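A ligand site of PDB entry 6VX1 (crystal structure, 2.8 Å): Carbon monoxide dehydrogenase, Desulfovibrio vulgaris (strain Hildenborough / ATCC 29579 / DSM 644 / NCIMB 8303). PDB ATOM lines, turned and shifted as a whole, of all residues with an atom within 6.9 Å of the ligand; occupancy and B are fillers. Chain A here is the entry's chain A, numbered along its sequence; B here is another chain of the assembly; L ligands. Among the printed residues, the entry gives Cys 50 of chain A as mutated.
The backbone NH (N) of Cys 74 lies close to a sulfur (S1) of the ligand (3.3 Å).
An iron atom (FE3) of the ligand is bound by the side-chain sulfur (SG) of Cys 74 (2.3 Å).
The side-chain sulfur of Cys 51 is bound to an iron atom (FE1) of the ligand (2.3 Å).
FE2 of the ligand is bound by SG of Cys 59, 2.3 Å away.
The side-chain sulfur of Cys 54 binds an iron atom (FE4) of the ligand (2.3 Å).
NH2 of Arg 84 sits close to S2 of the ligand, 3.5 Å away.
SG of Cys 74 lies close to N of Ala 76 (3.8 Å).
The backbone carbonyl oxygen of Cys 59 is in hydrogen-bond range of the backbone NH of Cys 51, 2.8 Å away.
NH2 of Arg 84 lies close to SG of Cys 51 (3.4 Å).
The side-chain sulfur of Cys 59 sits close to the backbone carbonyl oxygen of Gly 57 (3.2 Å).
The side-chain sulfur (SG) of Cys 59 lies close to the backbone NH (N) of Val 73 (3.5 Å).
The backbone NH of Met 56 lies close to the side-chain sulfur of Cys 54, 3.5 Å away.
ND2 of Asn 53 lies within hydrogen-bond range of O of Thr 201 (2.6 Å).
O of Gly 57 sits close to S3 of the ligand (3.0 Å).
Merely in contact with the ligand: Asn 53, Met 56, Gly 72, Val 73, Ile 81 and Met 203.
Hydrophobic or aromatic side chains that line the ligand: Met 56, Val 73, Ile 81 and Met 203.
Along chain A the residues within 4 Å of the ligand span positions 51 to 203.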
ATOM      1  N   CYS A  50      22.545  18.532 -28.110  1.00  0.00           N
ATOM      2  CA  CYS A  50      21.910  19.646 -27.440  1.00  0.00           C
ATOM      3  C   CYS A  50      22.974  20.486 -26.765  1.00  0.00           C
ATOM      4  O   CYS A  50      23.920  19.948 -26.173  1.00  0.00           O
ATOM      5  CB  CYS A  50      20.874  19.164 -26.416  1.00  0.00           C
ATOM      6  SG  CYS A  50      19.881  20.475 -25.667  1.00  0.00           S
ATOM      7  N   CYS A  51      22.835  21.804 -26.863  1.00  0.00           N
ATOM      8  CA  CYS A  51      23.808  22.743 -26.301  1.00  0.00           C
ATOM      9  C   CYS A  51      23.061  23.799 -25.510  1.00  0.00           C
ATOM     10  O   CYS A  51      22.175  24.471 -26.044  1.00  0.00           O
ATOM     11  CB  CYS A  51      24.655  23.387 -27.386  1.00  0.00           C
ATOM     12  SG  CYS A  51      25.915  24.503 -26.742  1.00  0.00           S
ATOM     13  N   ARG A  52      23.423  23.947 -24.235  1.00  0.00           N
ATOM     14  CA  ARG A  52      22.778  24.888 -23.320  1.00  0.00           C
ATOM     15  C   ARG A  52      23.781  25.869 -22.745  1.00  0.00           C
ATOM     16  O   ARG A  52      23.578  26.412 -21.657  1.00  0.00           O
ATOM     17  CB  ARG A  52      22.044  24.137 -22.211  1.00  0.00           C
ATOM     18  CG  ARG A  52      21.111  23.040 -22.738  1.00  0.00           C
ATOM     19  CD  ARG A  52      20.608  22.127 -21.634  1.00  0.00           C
ATOM     20  NE  ARG A  52      21.690  21.656 -20.782  1.00  0.00           N
ATOM     21  CZ  ARG A  52      21.601  20.619 -19.959  1.00  0.00           C
ATOM     22  NH1 ARG A  52      20.479  19.911 -19.896  1.00  0.00           N
ATOM     23  NH2 ARG A  52      22.645  20.258 -19.222  1.00  0.00           N
ATOM     24  N   ASN A  53      24.870  26.122 -23.460  1.00  0.00           N
ATOM     25  CA  ASN A  53      25.982  26.906 -22.937  1.00  0.00           C
ATOM     26  C   ASN A  53      25.747  28.420 -22.988  1.00  0.00           C
ATOM     27  O   ASN A  53      26.639  29.171 -22.547  1.00  0.00           O
ATOM     28  CB  ASN A  53      27.271  26.564 -23.690  1.00  0.00           C
ATOM     29  CG  ASN A  53      27.818  25.195 -23.315  1.00  0.00           C
ATOM     30  OD1 ASN A  53      27.103  24.371 -22.754  1.00  0.00           O
ATOM     31  ND2 ASN A  53      29.073  24.955 -23.631  1.00  0.00           N
ATOM     32  N   CYS A  54      24.617  28.884 -23.502  1.00  0.00           N
ATOM     33  CA  CYS A  54      24.279  30.296 -23.463  1.00  0.00           C
ATOM     34  C   CYS A  54      22.790  30.455 -23.761  1.00  0.00           C
ATOM     35  O   CYS A  54      22.133  29.518 -24.213  1.00  0.00           O
ATOM     36  CB  CYS A  54      25.136  31.107 -24.449  1.00  0.00           C
ATOM     37  SG  CYS A  54      24.543  31.100 -26.153  1.00  0.00           S
ATOM     38  N   ILE A  55      22.267  31.646 -23.486  1.00  0.00           N
ATOM     39  CA  ILE A  55      20.846  31.910 -23.672  1.00  0.00           C
ATOM     40  C   ILE A  55      20.578  32.720 -24.953  1.00  0.00           C
ATOM     41  O   ILE A  55      19.486  33.261 -25.112  1.00  0.00           O
ATOM     42  CB  ILE A  55      20.217  32.588 -22.442  1.00  0.00           C
ATOM     43  CG1 ILE A  55      20.877  33.938 -22.146  1.00  0.00           C
ATOM     44  CG2 ILE A  55      20.300  31.678 -21.224  1.00  0.00           C
ATOM     45  CD1 ILE A  55      19.876  35.056 -21.886  1.00  0.00           C
ATOM     46  N   MET A  56      21.540  32.788 -25.880  1.00  0.00           N
ATOM     47  CA  MET A  56      21.183  33.100 -27.258  1.00  0.00           C
ATOM     48  C   MET A  56      20.204  32.066 -27.789  1.00  0.00           C
ATOM     49  O   MET A  56      19.453  32.344 -28.732  1.00  0.00           O
ATOM     50  CB  MET A  56      22.405  33.183 -28.169  1.00  0.00           C
ATOM     51  CG  MET A  56      23.079  34.537 -28.186  1.00  0.00           C
ATOM     52  SD  MET A  56      23.943  34.951 -29.718  1.00  0.00           S
ATOM     53  CE  MET A  56      25.009  33.520 -29.925  1.00  0.00           C
ATOM     54  N   GLY A  57      20.213  30.877 -27.211  1.00  0.00           N
ATOM     55  CA  GLY A  57      19.129  29.942 -27.329  1.00  0.00           C
ATOM     56  C   GLY A  57      19.622  28.564 -26.987  1.00  0.00           C
ATOM     57  O   GLY A  57      20.749  28.197 -27.343  1.00  0.00           O
ATOM     58  N   PRO A  58      18.829  27.784 -26.269  1.00  0.00           N
ATOM     59  CA  PRO A  58      19.072  26.330 -26.259  1.00  0.00           C
ATOM     60  C   PRO A  58      19.034  25.816 -27.679  1.00  0.00           C
ATOM     61  O   PRO A  58      18.062  26.044 -28.415  1.00  0.00           O
ATOM     62  CB  PRO A  58      17.930  25.783 -25.406  1.00  0.00           C
ATOM     63  CG  PRO A  58      17.529  26.920 -24.530  1.00  0.00           C
ATOM     64  CD  PRO A  58      17.750  28.167 -25.351  1.00  0.00           C
ATOM     65  N   CYS A  59      20.113  25.164 -28.105  1.00  0.00           N
ATOM     66  CA  CYS A  59      20.262  24.729 -29.489  1.00  0.00           C
ATOM     67  C   CYS A  59      20.283  23.211 -29.578  1.00  0.00           C
ATOM     68  O   CYS A  59      20.867  22.540 -28.724  1.00  0.00           O
ATOM     69  CB  CYS A  59      21.532  25.305 -30.115  1.00  0.00           C
ATOM     70  SG  CYS A  59      21.589  27.102 -30.195  1.00  0.00           S
ATOM     71  N   ARG A  60      19.653  22.685 -30.619  1.00  0.00           N
ATOM     72  CA  ARG A  60      19.684  21.271 -30.946  1.00  0.00           C
ATOM     73  C   ARG A  60      20.144  21.129 -32.386  1.00  0.00           C
ATOM     74  O   ARG A  60      19.690  21.862 -33.267  1.00  0.00           O
ATOM     75  CB  ARG A  60      18.317  20.604 -30.760  1.00  0.00           C
ATOM     76  N   ILE A  61      21.058  20.198 -32.632  1.00  0.00           N
ATOM     77  CA  ILE A  61      21.514  19.868 -33.976  1.00  0.00           C
ATOM     78  C   ILE A  61      20.828  18.579 -34.410  1.00  0.00           C
ATOM     79  O   ILE A  61      21.034  17.526 -33.814  1.00  0.00           O
ATOM     80  CB  ILE A  61      23.046  19.724 -34.046  1.00  0.00           C
ATOM     81  CG1 ILE A  61      23.716  21.017 -33.578  1.00  0.00           C
ATOM     82  CG2 ILE A  61      23.486  19.421 -35.465  1.00  0.00           C
ATOM     83  CD1 ILE A  61      23.340  22.216 -34.388  1.00  0.00           C
ATOM     84  N   LEU A  71      22.998  24.132 -37.700  1.00  0.00           N
ATOM     85  CA  LEU A  71      23.975  24.844 -36.907  1.00  0.00           C
ATOM     86  C   LEU A  71      23.290  25.499 -35.718  1.00  0.00           C
ATOM     87  O   LEU A  71      22.078  25.735 -35.732  1.00  0.00           O
ATOM     88  CB  LEU A  71      24.712  25.912 -37.747  1.00  0.00           C
ATOM     89  CG  LEU A  71      25.461  25.409 -38.980  1.00  0.00           C
ATOM     90  CD1 LEU A  71      25.963  26.577 -39.801  1.00  0.00           C
ATOM     91  CD2 LEU A  71      26.608  24.488 -38.568  1.00  0.00           C
ATOM     92  N   GLY A  72      24.069  25.787 -34.685  1.00  0.00           N
ATOM     93  CA  GLY A  72      23.575  26.559 -33.563  1.00  0.00           C
ATOM     94  C   GLY A  72      23.437  28.031 -33.927  1.00  0.00           C
ATOM     95  O   GLY A  72      23.852  28.484 -34.981  1.00  0.00           O
ATOM     96  N   VAL A  73      22.827  28.788 -33.004  1.00  0.00           N
ATOM     97  CA  VAL A  73      22.625  30.219 -33.243  1.00  0.00           C
ATOM     98  C   VAL A  73      23.963  30.912 -33.464  1.00  0.00           C
ATOM     99  O   VAL A  73      24.107  31.776 -34.342  1.00  0.00           O
ATOM    100  CB  VAL A  73      21.841  30.859 -32.086  1.00  0.00           C
ATOM    101  CG1 VAL A  73      21.579  32.325 -32.379  1.00  0.00           C
ATOM    102  CG2 VAL A  73      20.538  30.133 -31.850  1.00  0.00           C
ATOM    103  N   CYS A  74      24.985  30.545 -32.672  1.00  0.00           N
ATOM    104  CA  CYS A  74      26.306  31.139 -32.835  1.00  0.00           C
ATOM    105  C   CYS A  74      27.023  30.612 -34.069  1.00  0.00           C
ATOM    106  O   CYS A  74      28.062  31.184 -34.443  1.00  0.00           O
ATOM    107  CB  CYS A  74      27.161  30.885 -31.596  1.00  0.00           C
ATOM    108  SG  CYS A  74      27.523  29.144 -31.277  1.00  0.00           S
ATOM    109  N   GLY A  75      26.525  29.554 -34.697  1.00  0.00           N
ATOM    110  CA  GLY A  75      27.157  28.971 -35.857  1.00  0.00           C
ATOM    111  C   GLY A  75      27.935  27.700 -35.614  1.00  0.00           C
ATOM    112  O   GLY A  75      28.641  27.235 -36.519  1.00  0.00           O
ATOM    113  N   ALA A  76      27.835  27.111 -34.422  1.00  0.00           N
ATOM    114  CA  ALA A  76      28.557  25.895 -34.097  1.00  0.00           C
ATOM    115  C   ALA A  76      27.902  24.681 -34.757  1.00  0.00           C
ATOM    116  O   ALA A  76      26.673  24.568 -34.782  1.00  0.00           O
ATOM    117  CB  ALA A  76      28.635  25.704 -32.594  1.00  0.00           C
ATOM    118  N   ASP A  77      28.736  23.776 -35.266  1.00  0.00           N
ATOM    119  CA  ASP A  77      28.247  22.570 -35.914  1.00  0.00           C
ATOM    120  C   ASP A  77      28.131  21.437 -34.891  1.00  0.00           C
ATOM    121  O   ASP A  77      28.391  21.611 -33.696  1.00  0.00           O
ATOM    122  CB  ASP A  77      29.148  22.178 -37.089  1.00  0.00           C
ATOM    123  CG  ASP A  77      30.580  21.817 -36.670  1.00  0.00           C
ATOM    124  OD1 ASP A  77      30.868  21.766 -35.463  1.00  0.00           O
ATOM    125  OD2 ASP A  77      31.412  21.585 -37.569  1.00  0.00           O
ATOM    126  N   ILE A  81      29.680  21.047 -30.897  1.00  0.00           N
ATOM    127  CA  ILE A  81      28.721  20.896 -29.811  1.00  0.00           C
ATOM    128  C   ILE A  81      28.928  19.578 -29.081  1.00  0.00           C
ATOM    129  O   ILE A  81      28.931  19.523 -27.837  1.00  0.00           O
ATOM    130  CB  ILE A  81      27.276  21.044 -30.332  1.00  0.00           C
ATOM    131  CG1 ILE A  81      27.002  22.513 -30.656  1.00  0.00           C
ATOM    132  CG2 ILE A  81      26.276  20.496 -29.326  1.00  0.00           C
ATOM    133  CD1 ILE A  81      25.593  22.778 -31.119  1.00  0.00           C
ATOM    134  N   ARG A  84      32.247  19.647 -27.079  1.00  0.00           N
ATOM    135  CA  ARG A  84      32.240  20.529 -25.922  1.00  0.00           C
ATOM    136  C   ARG A  84      31.517  19.878 -24.743  1.00  0.00           C
ATOM    137  O   ARG A  84      32.024  19.872 -23.621  1.00  0.00           O
ATOM    138  CB  ARG A  84      31.588  21.871 -26.272  1.00  0.00           C
ATOM    139  CG  ARG A  84      32.465  22.765 -27.128  1.00  0.00           C
ATOM    140  CD  ARG A  84      31.972  24.192 -27.166  1.00  0.00           C
ATOM    141  NE  ARG A  84      30.590  24.281 -27.588  1.00  0.00           N
ATOM    142  CZ  ARG A  84      30.044  25.387 -28.102  1.00  0.00           C
ATOM    143  NH1 ARG A  84      30.780  26.478 -28.257  1.00  0.00           N
ATOM    144  NH2 ARG A  84      28.763  25.402 -28.460  1.00  0.00           N
ATOM    145  N   THR A 201      34.982  25.445 -23.588  1.00  0.00           N
ATOM    146  CA  THR A 201      33.618  25.044 -23.922  1.00  0.00           C
ATOM    147  C   THR A 201      32.615  26.194 -23.852  1.00  0.00           C
ATOM    148  O   THR A 201      31.437  25.978 -24.146  1.00  0.00           O
ATOM    149  CB  THR A 201      33.177  23.905 -22.996  1.00  0.00           C
ATOM    150  OG1 THR A 201      33.372  24.293 -21.629  1.00  0.00           O
ATOM    151  CG2 THR A 201      34.007  22.667 -23.286  1.00  0.00           C
ATOM    152  N   HIS A 202      33.048  27.391 -23.461  1.00  0.00           N
ATOM    153  CA  HIS A 202      32.229  28.587 -23.523  1.00  0.00           C
ATOM    154  C   HIS A 202      31.967  28.960 -24.988  1.00  0.00           C
ATOM    155  O   HIS A 202      32.680  28.536 -25.897  1.00  0.00           O
ATOM    156  CB  HIS A 202      32.912  29.740 -22.774  1.00  0.00           C
ATOM    157  CG  HIS A 202      32.086  30.983 -22.656  1.00  0.00           C
ATOM    158  ND1 HIS A 202      32.068  31.958 -23.637  1.00  0.00           N
ATOM    159  CD2 HIS A 202      31.288  31.433 -21.661  1.00  0.00           C
ATOM    160  CE1 HIS A 202      31.268  32.944 -23.253  1.00  0.00           C
ATOM    161  NE2 HIS A 202      30.788  32.655 -22.059  1.00  0.00           N
ATOM    162  N   MET A 203      30.914  29.740 -25.202  1.00  0.00           N
ATOM    163  CA  MET A 203      30.571  30.182 -26.555  1.00  0.00           C
ATOM    164  C   MET A 203      31.727  30.949 -27.178  1.00  0.00           C
ATOM    165  O   MET A 203      32.310  31.840 -26.552  1.00  0.00           O
ATOM    166  CB  MET A 203      29.318  31.066 -26.525  1.00  0.00           C
ATOM    167  CG  MET A 203      28.711  31.347 -27.909  1.00  0.00           C
ATOM    168  SD  MET A 203      29.622  32.465 -29.012  1.00  0.00           S
ATOM    169  CE  MET A 203      28.639  33.962 -28.959  1.00  0.00           C
ATOM    170  N   GLY A 204      32.067  30.601 -28.412  1.00  0.00           N
ATOM    171  CA  GLY A 204      33.025  31.376 -29.174  1.00  0.00           C
ATOM    172  C   GLY A 204      34.455  31.286 -28.711  1.00  0.00           C
ATOM    173  O   GLY A 204      35.243  32.195 -28.999  1.00  0.00           O
ATOM    174  N   GLN B  38      16.160  27.911 -34.311  1.00  0.00           N
ATOM    175  CA  GLN B  38      16.378  27.271 -33.018  1.00  0.00           C
ATOM    176  C   GLN B  38      15.367  27.720 -31.962  1.00  0.00           C
ATOM    177  O   GLN B  38      15.664  27.656 -30.767  1.00  0.00           O
ATOM    178  CB  GLN B  38      17.799  27.548 -32.535  1.00  0.00           C
ATOM    179  CG  GLN B  38      18.885  26.879 -33.359  1.00  0.00           C
ATOM    180  CD  GLN B  38      18.884  25.375 -33.194  1.00  0.00           C
ATOM    181  OE1 GLN B  38      18.220  24.833 -32.319  1.00  0.00           O
ATOM    182  NE2 GLN B  38      19.648  24.690 -34.049  1.00  0.00           N
ATOM    183  N   PRO B 343      31.576  31.160 -34.527  1.00  0.00           N
ATOM    184  CA  PRO B 343      32.283  30.380 -35.565  1.00  0.00           C
ATOM    185  C   PRO B 343      31.675  30.510 -36.955  1.00  0.00           C
ATOM    186  O   PRO B 343      32.280  30.016 -37.913  1.00  0.00           O
ATOM    187  CB  PRO B 343      32.191  28.941 -35.039  1.00  0.00           C
ATOM    188  CG  PRO B 343      30.987  28.936 -34.161  1.00  0.00           C
ATOM    189  CD  PRO B 343      30.948  30.289 -33.521  1.00  0.00           C
ATOM    190  N   TYR B 553      23.504  37.290 -23.005  1.00  0.00           N
ATOM    191  CA  TYR B 553      23.363  35.941 -23.546  1.00  0.00           C
ATOM    192  C   TYR B 553      24.357  34.930 -22.979  1.00  0.00           C
ATOM    193  O   TYR B 553      24.015  33.746 -22.903  1.00  0.00           O
ATOM    194  CB  TYR B 553      23.501  35.956 -25.070  1.00  0.00           C
ATOM    195  CG  TYR B 553      24.936  36.108 -25.539  1.00  0.00           C
ATOM    196  CD1 TYR B 553      25.488  37.369 -25.727  1.00  0.00           C
ATOM    197  CD2 TYR B 553      25.735  34.997 -25.789  1.00  0.00           C
ATOM    198  CE1 TYR B 553      26.785  37.520 -26.142  1.00  0.00           C
ATOM    199  CE2 TYR B 553      27.043  35.148 -26.195  1.00  0.00           C
ATOM    200  CZ  TYR B 553      27.569  36.410 -26.372  1.00  0.00           C
ATOM    201  OH  TYR B 553      28.866  36.578 -26.788  1.00  0.00           O
HETATM  202 FE1  LIG L   1      25.520  26.535 -27.688  1.00  0.00          FE
HETATM  203 FE2  LIG L   1      23.541  27.686 -29.177  1.00  0.00          FE
HETATM  204 FE3  LIG L   1      26.162  28.368 -29.633  1.00  0.00          FE
HETATM  205 FE4  LIG L   1      24.901  29.179 -27.334  1.00  0.00          FE
HETATM  206  S1  LIG L   1      24.370  29.779 -29.471  1.00  0.00           S
HETATM  207  S2  LIG L   1      26.993  28.274 -27.503  1.00  0.00           S
HETATM  208  S3  LIG L   1      23.561  27.386 -26.911  1.00  0.00           S
HETATM  209  S4  LIG L   1      25.208  26.318 -29.946  1.00  0.00           S
